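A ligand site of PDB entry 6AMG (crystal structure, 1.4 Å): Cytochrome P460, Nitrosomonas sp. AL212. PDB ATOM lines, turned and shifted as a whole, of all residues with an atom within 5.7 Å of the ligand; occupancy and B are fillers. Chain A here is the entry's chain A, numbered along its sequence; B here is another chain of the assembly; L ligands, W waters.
ND1 of His 80 lies within hydrogen-bond range of O4 of the ligand (2.6 Å).
The side-chain sulfur (SG) of Cys 168 is bonded to a carbon (C18) of the ligand, 1.9 Å away.
A carbon (C1) of the ligand is bonded to the side-chain amino group (NZ) of Lys 106.
An oxygen (O1) of the ligand lies within hydrogen-bond range of the backbone NH of Phe 182.
An oxygen (O3) of the ligand lies within hydrogen-bond range of the side-chain hydroxyl (OG) of Ser 118 of chain B, at 2.6 Å.
A carbon (C25) of the ligand is covalently linked to the side-chain sulfur of Cys 171 (1.9 Å).
The side-chain hydroxyl of Tyr 186 lies within hydrogen-bond range of an oxygen (O2) of the ligand, 2.5 Å away.
A ring nitrogen (NE2) of His 172 binds an iron atom (FE1) of the ligand (2.2 Å).
The backbone NH (N) of Phe 150 lies within hydrogen-bond range of the backbone carbonyl oxygen (O) of Ala 132 (2.8 Å).
OG1 of Thr 167 sits at hydrogen-bond distance from OE2 of Glu 166 (2.8 Å).
The backbone NH of His 80 sits at hydrogen-bond distance from the backbone carbonyl oxygen of Ser 63 (2.8 Å).
A ring nitrogen (NE2) of His 80 is in hydrogen-bond range of the backbone carbonyl oxygen (O) of Phe 76, 2.7 Å away.
The side-chain hydroxyl of Tyr 186 lies within hydrogen-bond range of the side-chain amino group of Lys 106, at 3.3 Å.
The backbone carbonyl oxygen of Phe 76 lies within hydrogen-bond range of the side-chain hydroxyl of Thr 65 (3.1 Å).
O of Ala 131 is in hydrogen-bond range of N of Lys 106, at 2.8 Å.
OG of Ser 118 of chain B lies within hydrogen-bond range of OG of Ser 116 of chain B (2.9 Å).
Ser 63 touches the ligand.
Phe 76 touches the ligand.
Val 82 touches the ligand.
CG2 of Ile 104 touches C11 of the ligand (3.8 Å).
Ala 131 touches the ligand.
Ala 132 touches the ligand (O to C17, 3.9 Å).
Met 133 touches the ligand.
Phe 149 touches the ligand.
O of Phe 150 touches C17 of the ligand, 3.4 Å away.
Thr 167 touches the ligand.
Met 180 touches the ligand.
Val 181 touches the ligand (CA to O1, 3.2 Å).
Phe 185 touches the ligand.
Ser 116 of chain B touches the ligand.
Pro 117 of chain B touches the ligand (O to C26, 3.4 Å).
Phe 123 of chain B touches the ligand (CE1 to O3, 3.4 Å).
Of the 32 residues printed, 24 come within 4 Å of the ligand.
Water W1 lies within hydrogen-bond range of O4 of the ligand and OH of Tyr 186.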
ATOM      1  N   SER A  63     -26.692   0.350 -26.381  1.00  0.00           N
ATOM      2  CA  SER A  63     -25.375  -0.270 -26.223  1.00  0.00           C
ATOM      3  C   SER A  63     -25.039  -0.289 -24.740  1.00  0.00           C
ATOM      4  O   SER A  63     -25.739   0.302 -23.905  1.00  0.00           O
ATOM      5  CB  SER A  63     -24.282   0.513 -26.980  1.00  0.00           C
ATOM      6  OG  SER A  63     -24.496   0.436 -28.383  1.00  0.00           O
ATOM      7  N   THR A  65     -21.447  -0.034 -22.162  1.00  0.00           N
ATOM      8  CA  THR A  65     -20.022   0.026 -21.844  1.00  0.00           C
ATOM      9  C   THR A  65     -19.895  -0.109 -20.327  1.00  0.00           C
ATOM     10  O   THR A  65     -19.961   0.900 -19.590  1.00  0.00           O
ATOM     11  CB  THR A  65     -19.375   1.312 -22.355  1.00  0.00           C
ATOM     12  OG1 THR A  65     -20.063   2.469 -21.838  1.00  0.00           O
ATOM     13  CG2 THR A  65     -19.361   1.357 -23.871  1.00  0.00           C
ATOM     14  N   PHE A  76     -19.057   6.861 -20.384  1.00  0.00           N
ATOM     15  CA  PHE A  76     -20.500   7.040 -20.216  1.00  0.00           C
ATOM     16  C   PHE A  76     -20.983   5.786 -19.510  1.00  0.00           C
ATOM     17  O   PHE A  76     -21.349   4.791 -20.150  1.00  0.00           O
ATOM     18  CB  PHE A  76     -21.212   7.188 -21.572  1.00  0.00           C
ATOM     19  CG  PHE A  76     -21.218   8.588 -22.165  1.00  0.00           C
ATOM     20  CD1 PHE A  76     -20.600   9.658 -21.567  1.00  0.00           C
ATOM     21  CD2 PHE A  76     -21.885   8.813 -23.346  1.00  0.00           C
ATOM     22  CE1 PHE A  76     -20.657  10.924 -22.161  1.00  0.00           C
ATOM     23  CE2 PHE A  76     -21.942  10.063 -23.933  1.00  0.00           C
ATOM     24  CZ  PHE A  76     -21.324  11.100 -23.340  1.00  0.00           C
ATOM     25  N   HIS A  80     -26.516   2.618 -22.500  1.00  0.00           N
ATOM     26  CA  HIS A  80     -26.925   3.831 -23.215  1.00  0.00           C
ATOM     27  C   HIS A  80     -28.192   3.498 -23.997  1.00  0.00           C
ATOM     28  O   HIS A  80     -28.157   2.649 -24.884  1.00  0.00           O
ATOM     29  CB  HIS A  80     -25.860   4.274 -24.222  1.00  0.00           C
ATOM     30  CG  HIS A  80     -24.474   4.303 -23.663  1.00  0.00           C
ATOM     31  ND1 HIS A  80     -23.369   4.154 -24.468  1.00  0.00           N
ATOM     32  CD2 HIS A  80     -24.008   4.425 -22.400  1.00  0.00           C
ATOM     33  CE1 HIS A  80     -22.280   4.190 -23.721  1.00  0.00           C
ATOM     34  NE2 HIS A  80     -22.643   4.347 -22.471  1.00  0.00           N
ATOM     35  N   VAL A  82     -30.888   5.266 -26.517  1.00  0.00           N
ATOM     36  CA  VAL A  82     -30.829   6.469 -27.350  1.00  0.00           C
ATOM     37  C   VAL A  82     -32.162   6.722 -28.039  1.00  0.00           C
ATOM     38  O   VAL A  82     -32.813   5.802 -28.538  1.00  0.00           O
ATOM     39  CB  VAL A  82     -29.682   6.339 -28.361  1.00  0.00           C
ATOM     40  CG1 VAL A  82     -29.500   7.648 -29.113  1.00  0.00           C
ATOM     41  CG2 VAL A  82     -28.396   5.924 -27.631  1.00  0.00           C
ATOM     42  N   ILE A 104     -31.207  14.421 -30.407  1.00  0.00           N
ATOM     43  CA  ILE A 104     -30.939  13.043 -30.011  1.00  0.00           C
ATOM     44  C   ILE A 104     -30.494  13.075 -28.562  1.00  0.00           C
ATOM     45  O   ILE A 104     -29.629  13.873 -28.190  1.00  0.00           O
ATOM     46  CB  ILE A 104     -29.874  12.386 -30.906  1.00  0.00           C
ATOM     47  CG1 ILE A 104     -30.436  12.193 -32.319  1.00  0.00           C
ATOM     48  CG2 ILE A 104     -29.455  11.023 -30.343  1.00  0.00           C
ATOM     49  CD1 ILE A 104     -29.417  11.794 -33.350  1.00  0.00           C
ATOM     50  N   VAL A 105     -31.096  12.208 -27.740  1.00  0.00           N
ATOM     51  CA  VAL A 105     -30.785  12.097 -26.320  1.00  0.00           C
ATOM     52  C   VAL A 105     -30.244  10.702 -26.078  1.00  0.00           C
ATOM     53  O   VAL A 105     -30.878   9.711 -26.436  1.00  0.00           O
ATOM     54  CB  VAL A 105     -32.022  12.331 -25.433  1.00  0.00           C
ATOM     55  CG1 VAL A 105     -31.729  12.001 -23.976  1.00  0.00           C
ATOM     56  CG2 VAL A 105     -32.506  13.766 -25.569  1.00  0.00           C
ATOM     57  N   LYS A 106     -29.077  10.636 -25.445  1.00  0.00           N
ATOM     58  CA  LYS A 106     -28.494   9.384 -24.983  1.00  0.00           C
ATOM     59  C   LYS A 106     -28.705   9.332 -23.485  1.00  0.00           C
ATOM     60  O   LYS A 106     -28.142  10.144 -22.741  1.00  0.00           O
ATOM     61  CB  LYS A 106     -27.016   9.311 -25.341  1.00  0.00           C
ATOM     62  CG  LYS A 106     -26.308   8.105 -24.744  1.00  0.00           C
ATOM     63  CD  LYS A 106     -24.982   7.800 -25.484  1.00  0.00           C
ATOM     64  CE  LYS A 106     -25.226   7.173 -26.824  1.00  0.00           C
ATOM     65  NZ  LYS A 106     -24.066   6.985 -27.712  1.00  0.00           N
ATOM     66  N   ALA A 131     -26.909  12.647 -22.085  1.00  0.00           N
ATOM     67  CA  ALA A 131     -26.147  13.496 -22.977  1.00  0.00           C
ATOM     68  C   ALA A 131     -27.039  13.787 -24.181  1.00  0.00           C
ATOM     69  O   ALA A 131     -27.990  13.054 -24.439  1.00  0.00           O
ATOM     70  CB  ALA A 131     -24.878  12.793 -23.452  1.00  0.00           C
ATOM     71  N   ALA A 132     -26.754  14.863 -24.903  1.00  0.00           N
ATOM     72  CA  ALA A 132     -27.600  15.168 -26.051  1.00  0.00           C
ATOM     73  C   ALA A 132     -26.824  15.889 -27.148  1.00  0.00           C
ATOM     74  O   ALA A 132     -25.736  16.420 -26.939  1.00  0.00           O
ATOM     75  CB  ALA A 132     -28.806  16.032 -25.651  1.00  0.00           C
ATOM     76  N   MET A 133     -27.421  15.876 -28.347  1.00  0.00           N
ATOM     77  CA  MET A 133     -26.877  16.619 -29.471  1.00  0.00           C
ATOM     78  C   MET A 133     -28.043  17.195 -30.272  1.00  0.00           C
ATOM     79  O   MET A 133     -29.105  16.582 -30.355  1.00  0.00           O
ATOM     80  CB  MET A 133     -25.957  15.743 -30.337  1.00  0.00           C
ATOM     81  CG  MET A 133     -26.588  14.526 -30.968  1.00  0.00           C
ATOM     82  SD  MET A 133     -25.391  13.303 -31.569  1.00  0.00           S
ATOM     83  CE  MET A 133     -24.773  14.107 -33.032  1.00  0.00           C
ATOM     84  N   PHE A 149     -23.220  19.722 -29.060  1.00  0.00           N
ATOM     85  CA  PHE A 149     -23.189  18.644 -28.084  1.00  0.00           C
ATOM     86  C   PHE A 149     -23.388  19.219 -26.693  1.00  0.00           C
ATOM     87  O   PHE A 149     -22.747  20.214 -26.340  1.00  0.00           O
ATOM     88  CB  PHE A 149     -21.876  17.876 -28.172  1.00  0.00           C
ATOM     89  CG  PHE A 149     -21.769  17.024 -29.391  1.00  0.00           C
ATOM     90  CD1 PHE A 149     -21.416  17.578 -30.623  1.00  0.00           C
ATOM     91  CD2 PHE A 149     -22.072  15.676 -29.341  1.00  0.00           C
ATOM     92  CE1 PHE A 149     -21.343  16.777 -31.758  1.00  0.00           C
ATOM     93  CE2 PHE A 149     -21.992  14.887 -30.458  1.00  0.00           C
ATOM     94  CZ  PHE A 149     -21.634  15.421 -31.678  1.00  0.00           C
ATOM     95  N   PHE A 150     -24.269  18.590 -25.918  1.00  0.00           N
ATOM     96  CA  PHE A 150     -24.642  19.071 -24.594  1.00  0.00           C
ATOM     97  C   PHE A 150     -24.368  18.013 -23.544  1.00  0.00           C
ATOM     98  O   PHE A 150     -24.851  16.880 -23.645  1.00  0.00           O
ATOM     99  CB  PHE A 150     -26.123  19.464 -24.567  1.00  0.00           C
ATOM    100  CG  PHE A 150     -26.417  20.644 -25.407  1.00  0.00           C
ATOM    101  CD1 PHE A 150     -26.251  21.932 -24.927  1.00  0.00           C
ATOM    102  CD2 PHE A 150     -26.824  20.481 -26.712  1.00  0.00           C
ATOM    103  CE1 PHE A 150     -26.478  23.015 -25.725  1.00  0.00           C
ATOM    104  CE2 PHE A 150     -27.058  21.576 -27.511  1.00  0.00           C
ATOM    105  CZ  PHE A 150     -26.885  22.843 -27.017  1.00  0.00           C
ATOM    106  N   GLY A 151     -23.629  18.414 -22.518  1.00  0.00           N
ATOM    107  CA  GLY A 151     -23.492  17.647 -21.299  1.00  0.00           C
ATOM    108  C   GLY A 151     -24.476  18.147 -20.255  1.00  0.00           C
ATOM    109  O   GLY A 151     -24.907  19.302 -20.276  1.00  0.00           O
ATOM    110  N   GLN A 163     -20.638  22.026 -25.412  1.00  0.00           N
ATOM    111  CA  GLN A 163     -19.260  21.568 -25.294  1.00  0.00           C
ATOM    112  C   GLN A 163     -18.391  22.128 -26.415  1.00  0.00           C
ATOM    113  O   GLN A 163     -18.870  22.340 -27.547  1.00  0.00           O
ATOM    114  CB  GLN A 163     -19.216  20.034 -25.361  1.00  0.00           C
ATOM    115  CG  GLN A 163     -20.090  19.404 -24.279  1.00  0.00           C
ATOM    116  CD  GLN A 163     -19.504  19.617 -22.894  1.00  0.00           C
ATOM    117  OE1 GLN A 163     -18.348  19.278 -22.643  1.00  0.00           O
ATOM    118  NE2 GLN A 163     -20.294  20.194 -21.989  1.00  0.00           N
ATOM    119  N   GLU A 166     -13.442  19.529 -29.120  1.00  0.00           N
ATOM    120  CA  GLU A 166     -12.573  18.406 -28.780  1.00  0.00           C
ATOM    121  C   GLU A 166     -13.220  17.424 -27.825  1.00  0.00           C
ATOM    122  O   GLU A 166     -12.808  16.262 -27.759  1.00  0.00           O
ATOM    123  CB  GLU A 166     -11.252  18.883 -28.154  1.00  0.00           C
ATOM    124  CG  GLU A 166     -11.279  19.149 -26.634  1.00  0.00           C
ATOM    125  CD  GLU A 166     -12.063  20.364 -26.247  1.00  0.00           C
ATOM    126  OE1 GLU A 166     -12.386  21.152 -27.132  1.00  0.00           O
ATOM    127  OE2 GLU A 166     -12.310  20.560 -25.030  1.00  0.00           O
ATOM    128  N   THR A 167     -14.234  17.841 -27.071  1.00  0.00           N
ATOM    129  CA  THR A 167     -14.767  17.002 -26.019  1.00  0.00           C
ATOM    130  C   THR A 167     -15.759  15.978 -26.528  1.00  0.00           C
ATOM    131  O   THR A 167     -15.924  14.932 -25.897  1.00  0.00           O
ATOM    132  CB  THR A 167     -15.395  17.908 -24.966  1.00  0.00           C
ATOM    133  OG1 THR A 167     -14.384  18.824 -24.528  1.00  0.00           O
ATOM    134  CG2 THR A 167     -15.888  17.159 -23.756  1.00  0.00           C
ATOM    135  N   CYS A 168     -16.422  16.249 -27.669  1.00  0.00           N
ATOM    136  CA  CYS A 168     -17.494  15.370 -28.129  1.00  0.00           C
ATOM    137  C   CYS A 168     -17.481  15.292 -29.643  1.00  0.00           C
ATOM    138  O   CYS A 168     -17.370  14.213 -30.219  1.00  0.00           O
ATOM    139  CB  CYS A 168     -18.875  15.893 -27.699  1.00  0.00           C
ATOM    140  SG  CYS A 168     -19.018  16.527 -25.998  1.00  0.00           S
ATOM    141  N   CYS A 171     -14.696  13.214 -31.765  1.00  0.00           N
ATOM    142  CA  CYS A 171     -14.850  11.756 -31.830  1.00  0.00           C
ATOM    143  C   CYS A 171     -16.007  11.378 -32.753  1.00  0.00           C
ATOM    144  O   CYS A 171     -15.870  10.476 -33.592  1.00  0.00           O
ATOM    145  CB  CYS A 171     -15.087  11.188 -30.427  1.00  0.00           C
ATOM    146  SG  CYS A 171     -15.293   9.400 -30.488  1.00  0.00           S
ATOM    147  N   HIS A 172     -17.139  12.064 -32.621  1.00  0.00           N
ATOM    148  CA  HIS A 172     -18.272  11.761 -33.475  1.00  0.00           C
ATOM    149  C   HIS A 172     -17.926  12.020 -34.950  1.00  0.00           C
ATOM    150  O   HIS A 172     -18.246  11.215 -35.835  1.00  0.00           O
ATOM    151  CB  HIS A 172     -19.503  12.565 -33.023  1.00  0.00           C
ATOM    152  CG  HIS A 172     -20.195  11.997 -31.808  1.00  0.00           C
ATOM    153  ND1 HIS A 172     -21.448  11.438 -31.878  1.00  0.00           N
ATOM    154  CD2 HIS A 172     -19.798  11.870 -30.504  1.00  0.00           C
ATOM    155  CE1 HIS A 172     -21.805  11.001 -30.677  1.00  0.00           C
ATOM    156  NE2 HIS A 172     -20.827  11.257 -29.833  1.00  0.00           N
ATOM    157  N   HIS A 175     -15.546   9.205 -36.325  1.00  0.00           N
ATOM    158  CA  HIS A 175     -15.914   7.797 -36.262  1.00  0.00           C
ATOM    159  C   HIS A 175     -17.363   7.464 -36.552  1.00  0.00           C
ATOM    160  O   HIS A 175     -17.644   6.288 -36.812  1.00  0.00           O
ATOM    161  CB  HIS A 175     -15.568   7.232 -34.882  1.00  0.00           C
ATOM    162  CG  HIS A 175     -14.115   7.268 -34.561  1.00  0.00           C
ATOM    163  ND1 HIS A 175     -13.177   6.558 -35.279  1.00  0.00           N
ATOM    164  CD2 HIS A 175     -13.437   7.876 -33.561  1.00  0.00           C
ATOM    165  CE1 HIS A 175     -11.994   6.740 -34.743  1.00  0.00           C
ATOM    166  NE2 HIS A 175     -12.119   7.523 -33.693  1.00  0.00           N
ATOM    167  N   ALA A 176     -18.289   8.416 -36.499  1.00  0.00           N
ATOM    168  CA  ALA A 176     -19.701   8.092 -36.712  1.00  0.00           C
ATOM    169  C   ALA A 176     -19.963   7.773 -38.170  1.00  0.00           C
ATOM    170  O   ALA A 176     -19.428   8.402 -39.073  1.00  0.00           O
ATOM    171  CB  ALA A 176     -20.581   9.264 -36.284  1.00  0.00           C
ATOM    172  N   MET A 180     -22.306  12.525 -38.167  1.00  0.00           N
ATOM    173  CA  MET A 180     -21.899  12.621 -36.781  1.00  0.00           C
ATOM    174  C   MET A 180     -22.696  11.816 -35.794  1.00  0.00           C
ATOM    175  O   MET A 180     -22.454  11.939 -34.581  1.00  0.00           O
ATOM    176  CB  MET A 180     -21.728  14.046 -36.343  1.00  0.00           C
ATOM    177  CG  MET A 180     -20.377  14.370 -36.887  1.00  0.00           C
ATOM    178  SD  MET A 180     -19.999  15.993 -36.857  1.00  0.00           S
ATOM    179  CE  MET A 180     -19.871  16.287 -35.118  1.00  0.00           C
ATOM    180  N   VAL A 181     -23.583  10.968 -36.271  1.00  0.00           N
ATOM    181  CA  VAL A 181     -24.363  10.074 -35.437  1.00  0.00           C
ATOM    182  C   VAL A 181     -23.879   8.655 -35.702  1.00  0.00           C
ATOM    183  O   VAL A 181     -23.730   8.237 -36.863  1.00  0.00           O
ATOM    184  CB  VAL A 181     -25.860  10.244 -35.707  1.00  0.00           C
ATOM    185  CG1 VAL A 181     -26.674   9.239 -34.908  1.00  0.00           C
ATOM    186  CG2 VAL A 181     -26.285  11.667 -35.375  1.00  0.00           C
ATOM    187  N   PHE A 182     -23.662   7.901 -34.622  1.00  0.00           N
ATOM    188  CA  PHE A 182     -23.125   6.538 -34.733  1.00  0.00           C
ATOM    189  C   PHE A 182     -24.198   5.537 -35.191  1.00  0.00           C
ATOM    190  O   PHE A 182     -24.551   4.599 -34.500  1.00  0.00           O
ATOM    191  CB  PHE A 182     -22.498   6.113 -33.401  1.00  0.00           C
ATOM    192  CG  PHE A 182     -21.150   6.728 -33.158  1.00  0.00           C
ATOM    193  CD1 PHE A 182     -20.006   6.123 -33.661  1.00  0.00           C
ATOM    194  CD2 PHE A 182     -21.011   7.870 -32.393  1.00  0.00           C
ATOM    195  CE1 PHE A 182     -18.756   6.682 -33.430  1.00  0.00           C
ATOM    196  CE2 PHE A 182     -19.783   8.425 -32.157  1.00  0.00           C
ATOM    197  CZ  PHE A 182     -18.645   7.824 -32.684  1.00  0.00           C
ATOM    198  N   THR A 183     -24.678   5.743 -36.422  1.00  0.00           N
ATOM    199  CA  THR A 183     -25.760   4.919 -36.948  1.00  0.00           C
ATOM    200  C   THR A 183     -25.375   3.467 -37.114  1.00  0.00           C
ATOM    201  O   THR A 183     -26.271   2.626 -37.262  1.00  0.00           O
ATOM    202  CB  THR A 183     -26.280   5.503 -38.276  1.00  0.00           C
ATOM    203  OG1 THR A 183     -25.220   5.564 -39.234  1.00  0.00           O
ATOM    204  CG2 THR A 183     -26.880   6.877 -38.077  1.00  0.00           C
ATOM    205  N   PHE A 185     -24.644   1.756 -34.762  1.00  0.00           N
ATOM    206  CA  PHE A 185     -25.188   1.200 -33.519  1.00  0.00           C
ATOM    207  C   PHE A 185     -26.673   1.493 -33.346  1.00  0.00           C
ATOM    208  O   PHE A 185     -27.210   1.231 -32.272  1.00  0.00           O
ATOM    209  CB  PHE A 185     -24.390   1.709 -32.311  1.00  0.00           C
ATOM    210  CG  PHE A 185     -22.902   1.445 -32.439  1.00  0.00           C
ATOM    211  CD1 PHE A 185     -22.418   0.200 -32.783  1.00  0.00           C
ATOM    212  CD2 PHE A 185     -21.982   2.459 -32.207  1.00  0.00           C
ATOM    213  CE1 PHE A 185     -21.057  -0.030 -32.914  1.00  0.00           C
ATOM    214  CE2 PHE A 185     -20.622   2.237 -32.315  1.00  0.00           C
ATOM    215  CZ  PHE A 185     -20.152   0.992 -32.677  1.00  0.00           C
ATOM    216  N   TYR A 186     -27.362   1.991 -34.395  1.00  0.00           N
ATOM    217  CA  TYR A 186     -28.788   2.327 -34.334  1.00  0.00           C
ATOM    218  C   TYR A 186     -29.527   1.509 -35.403  1.00  0.00           C
ATOM    219  O   TYR A 186     -29.839   2.015 -36.478  1.00  0.00           O
ATOM    220  CB  TYR A 186     -29.062   3.842 -34.433  1.00  0.00           C
ATOM    221  CG  TYR A 186     -28.328   4.538 -33.309  1.00  0.00           C
ATOM    222  CD1 TYR A 186     -28.522   4.127 -31.994  1.00  0.00           C
ATOM    223  CD2 TYR A 186     -27.411   5.546 -33.551  1.00  0.00           C
ATOM    224  CE1 TYR A 186     -27.810   4.666 -30.960  1.00  0.00           C
ATOM    225  CE2 TYR A 186     -26.670   6.085 -32.533  1.00  0.00           C
ATOM    226  CZ  TYR A 186     -26.863   5.641 -31.240  1.00  0.00           C
ATOM    227  OH  TYR A 186     -26.101   6.159 -30.226  1.00  0.00           O
ATOM    228  N   SER B 116     -15.673   0.007 -29.315  1.00  0.00           N
ATOM    229  CA  SER B 116     -15.983   1.172 -30.133  1.00  0.00           C
ATOM    230  C   SER B 116     -15.244   2.359 -29.540  1.00  0.00           C
ATOM    231  O   SER B 116     -14.550   2.221 -28.522  1.00  0.00           O
ATOM    232  CB  SER B 116     -17.489   1.433 -30.163  1.00  0.00           C
ATOM    233  OG  SER B 116     -17.871   2.360 -29.179  1.00  0.00           O
ATOM    234  N   PRO B 117     -15.363   3.539 -30.154  1.00  0.00           N
ATOM    235  CA  PRO B 117     -14.702   4.707 -29.555  1.00  0.00           C
ATOM    236  C   PRO B 117     -15.159   5.039 -28.159  1.00  0.00           C
ATOM    237  O   PRO B 117     -14.411   5.734 -27.445  1.00  0.00           O
ATOM    238  CB  PRO B 117     -15.045   5.844 -30.530  1.00  0.00           C
ATOM    239  CG  PRO B 117     -15.269   5.131 -31.850  1.00  0.00           C
ATOM    240  CD  PRO B 117     -15.965   3.851 -31.459  1.00  0.00           C
ATOM    241  N   SER B 118     -16.340   4.584 -27.733  1.00  0.00           N
ATOM    242  CA  SER B 118     -16.822   4.883 -26.395  1.00  0.00           C
ATOM    243  C   SER B 118     -16.320   3.888 -25.354  1.00  0.00           C
ATOM    244  O   SER B 118     -16.565   4.092 -24.166  1.00  0.00           O
ATOM    245  CB  SER B 118     -18.340   4.855 -26.373  1.00  0.00           C
ATOM    246  OG  SER B 118     -18.798   3.581 -26.747  1.00  0.00           O
ATOM    247  N   PHE B 123     -22.221  -3.826 -28.384  1.00  0.00           N
ATOM    248  CA  PHE B 123     -22.847  -2.876 -29.277  1.00  0.00           C
ATOM    249  C   PHE B 123     -23.691  -3.683 -30.261  1.00  0.00           C
ATOM    250  O   PHE B 123     -23.263  -4.754 -30.705  1.00  0.00           O
ATOM    251  CB  PHE B 123     -21.783  -2.077 -30.025  1.00  0.00           C
ATOM    252  CG  PHE B 123     -20.850  -1.370 -29.101  1.00  0.00           C
ATOM    253  CD1 PHE B 123     -21.167  -0.103 -28.602  1.00  0.00           C
ATOM    254  CD2 PHE B 123     -19.655  -1.972 -28.709  1.00  0.00           C
ATOM    255  CE1 PHE B 123     -20.325   0.526 -27.712  1.00  0.00           C
ATOM    256  CE2 PHE B 123     -18.792  -1.322 -27.813  1.00  0.00           C
ATOM    257  CZ  PHE B 123     -19.130  -0.076 -27.320  1.00  0.00           C
HETATM  258 FE1  LIG L   1     -20.790  10.451 -27.809  1.00  0.00          FE
HETATM  259  C1  LIG L   1     -23.242   7.985 -28.145  1.00  0.00           C
HETATM  260  C2  LIG L   1     -23.161  12.695 -26.931  1.00  0.00           C
HETATM  261  C3  LIG L   1     -18.410  12.357 -26.378  1.00  0.00           C
HETATM  262  C4  LIG L   1     -18.417   8.274 -28.805  1.00  0.00           C
HETATM  263  N1  LIG L   1     -22.843  10.390 -27.644  1.00  0.00           N
HETATM  264  C5  LIG L   1     -23.655   9.333 -28.094  1.00  0.00           C
HETATM  265  C6  LIG L   1     -24.940   9.929 -28.411  1.00  0.00           C
HETATM  266  C7  LIG L   1     -24.912  11.208 -27.981  1.00  0.00           C
HETATM  267  C8  LIG L   1     -23.588  11.522 -27.525  1.00  0.00           C
HETATM  268  C9  LIG L   1     -26.023  12.174 -28.120  1.00  0.00           C
HETATM  269  C10 LIG L   1     -25.969   9.261 -29.273  1.00  0.00           C
HETATM  270  C11 LIG L   1     -25.927   9.584 -30.753  1.00  0.00           C
HETATM  271  C12 LIG L   1     -24.724   8.874 -31.400  1.00  0.00           C
HETATM  272  O1  LIG L   1     -24.110   9.515 -32.316  1.00  0.00           O
HETATM  273  O2  LIG L   1     -24.366   7.723 -31.066  1.00  0.00           O
HETATM  274  N2  LIG L   1     -20.800  12.168 -26.778  1.00  0.00           N
HETATM  275  C13 LIG L   1     -21.970  12.972 -26.501  1.00  0.00           C
HETATM  276  C14 LIG L   1     -21.467  14.107 -25.773  1.00  0.00           C
HETATM  277  C15 LIG L   1     -20.126  13.989 -25.608  1.00  0.00           C
HETATM  278  C16 LIG L   1     -19.659  12.816 -26.203  1.00  0.00           C
HETATM  279  C17 LIG L   1     -22.385  15.227 -25.306  1.00  0.00           C
HETATM  280  C18 LIG L   1     -19.132  14.967 -24.923  1.00  0.00           C
HETATM  281  C19 LIG L   1     -19.598  15.470 -23.583  1.00  0.00           C
HETATM  282  N3  LIG L   1     -18.711  10.417 -27.635  1.00  0.00           N
HETATM  283  C20 LIG L   1     -17.911  11.355 -27.027  1.00  0.00           C
HETATM  284  C21 LIG L   1     -16.600  10.928 -27.354  1.00  0.00           C
HETATM  285  C22 LIG L   1     -16.579   9.830 -28.069  1.00  0.00           C
HETATM  286  C23 LIG L   1     -17.947   9.389 -28.213  1.00  0.00           C
HETATM  287  C24 LIG L   1     -15.457  11.821 -26.785  1.00  0.00           C
HETATM  288  C25 LIG L   1     -15.458   8.955 -28.672  1.00  0.00           C
HETATM  289  C26 LIG L   1     -14.049   9.075 -28.032  1.00  0.00           C
HETATM  290  N4  LIG L   1     -20.802   8.477 -28.426  1.00  0.00           N
HETATM  291  C27 LIG L   1     -19.677   7.801 -28.877  1.00  0.00           C
HETATM  292  C28 LIG L   1     -20.183   6.557 -29.353  1.00  0.00           C
HETATM  293  C29 LIG L   1     -21.498   6.381 -29.117  1.00  0.00           C
HETATM  294  C30 LIG L   1     -21.970   7.590 -28.540  1.00  0.00           C
HETATM  295  C31 LIG L   1     -19.239   5.515 -29.988  1.00  0.00           C
HETATM  296  C32 LIG L   1     -22.311   5.243 -29.571  1.00  0.00           C
HETATM  297  C33 LIG L   1     -22.027   3.892 -28.890  1.00  0.00           C
HETATM  298  C34 LIG L   1     -22.307   3.924 -27.521  1.00  0.00           C
HETATM  299  O3  LIG L   1     -21.421   3.609 -26.641  1.00  0.00           O
HETATM  300  O4  LIG L   1     -23.440   4.244 -27.097  1.00  0.00           O
HETATM  301  O   HOH W   1     -25.681   3.930 -28.538  1.00  0.00           O
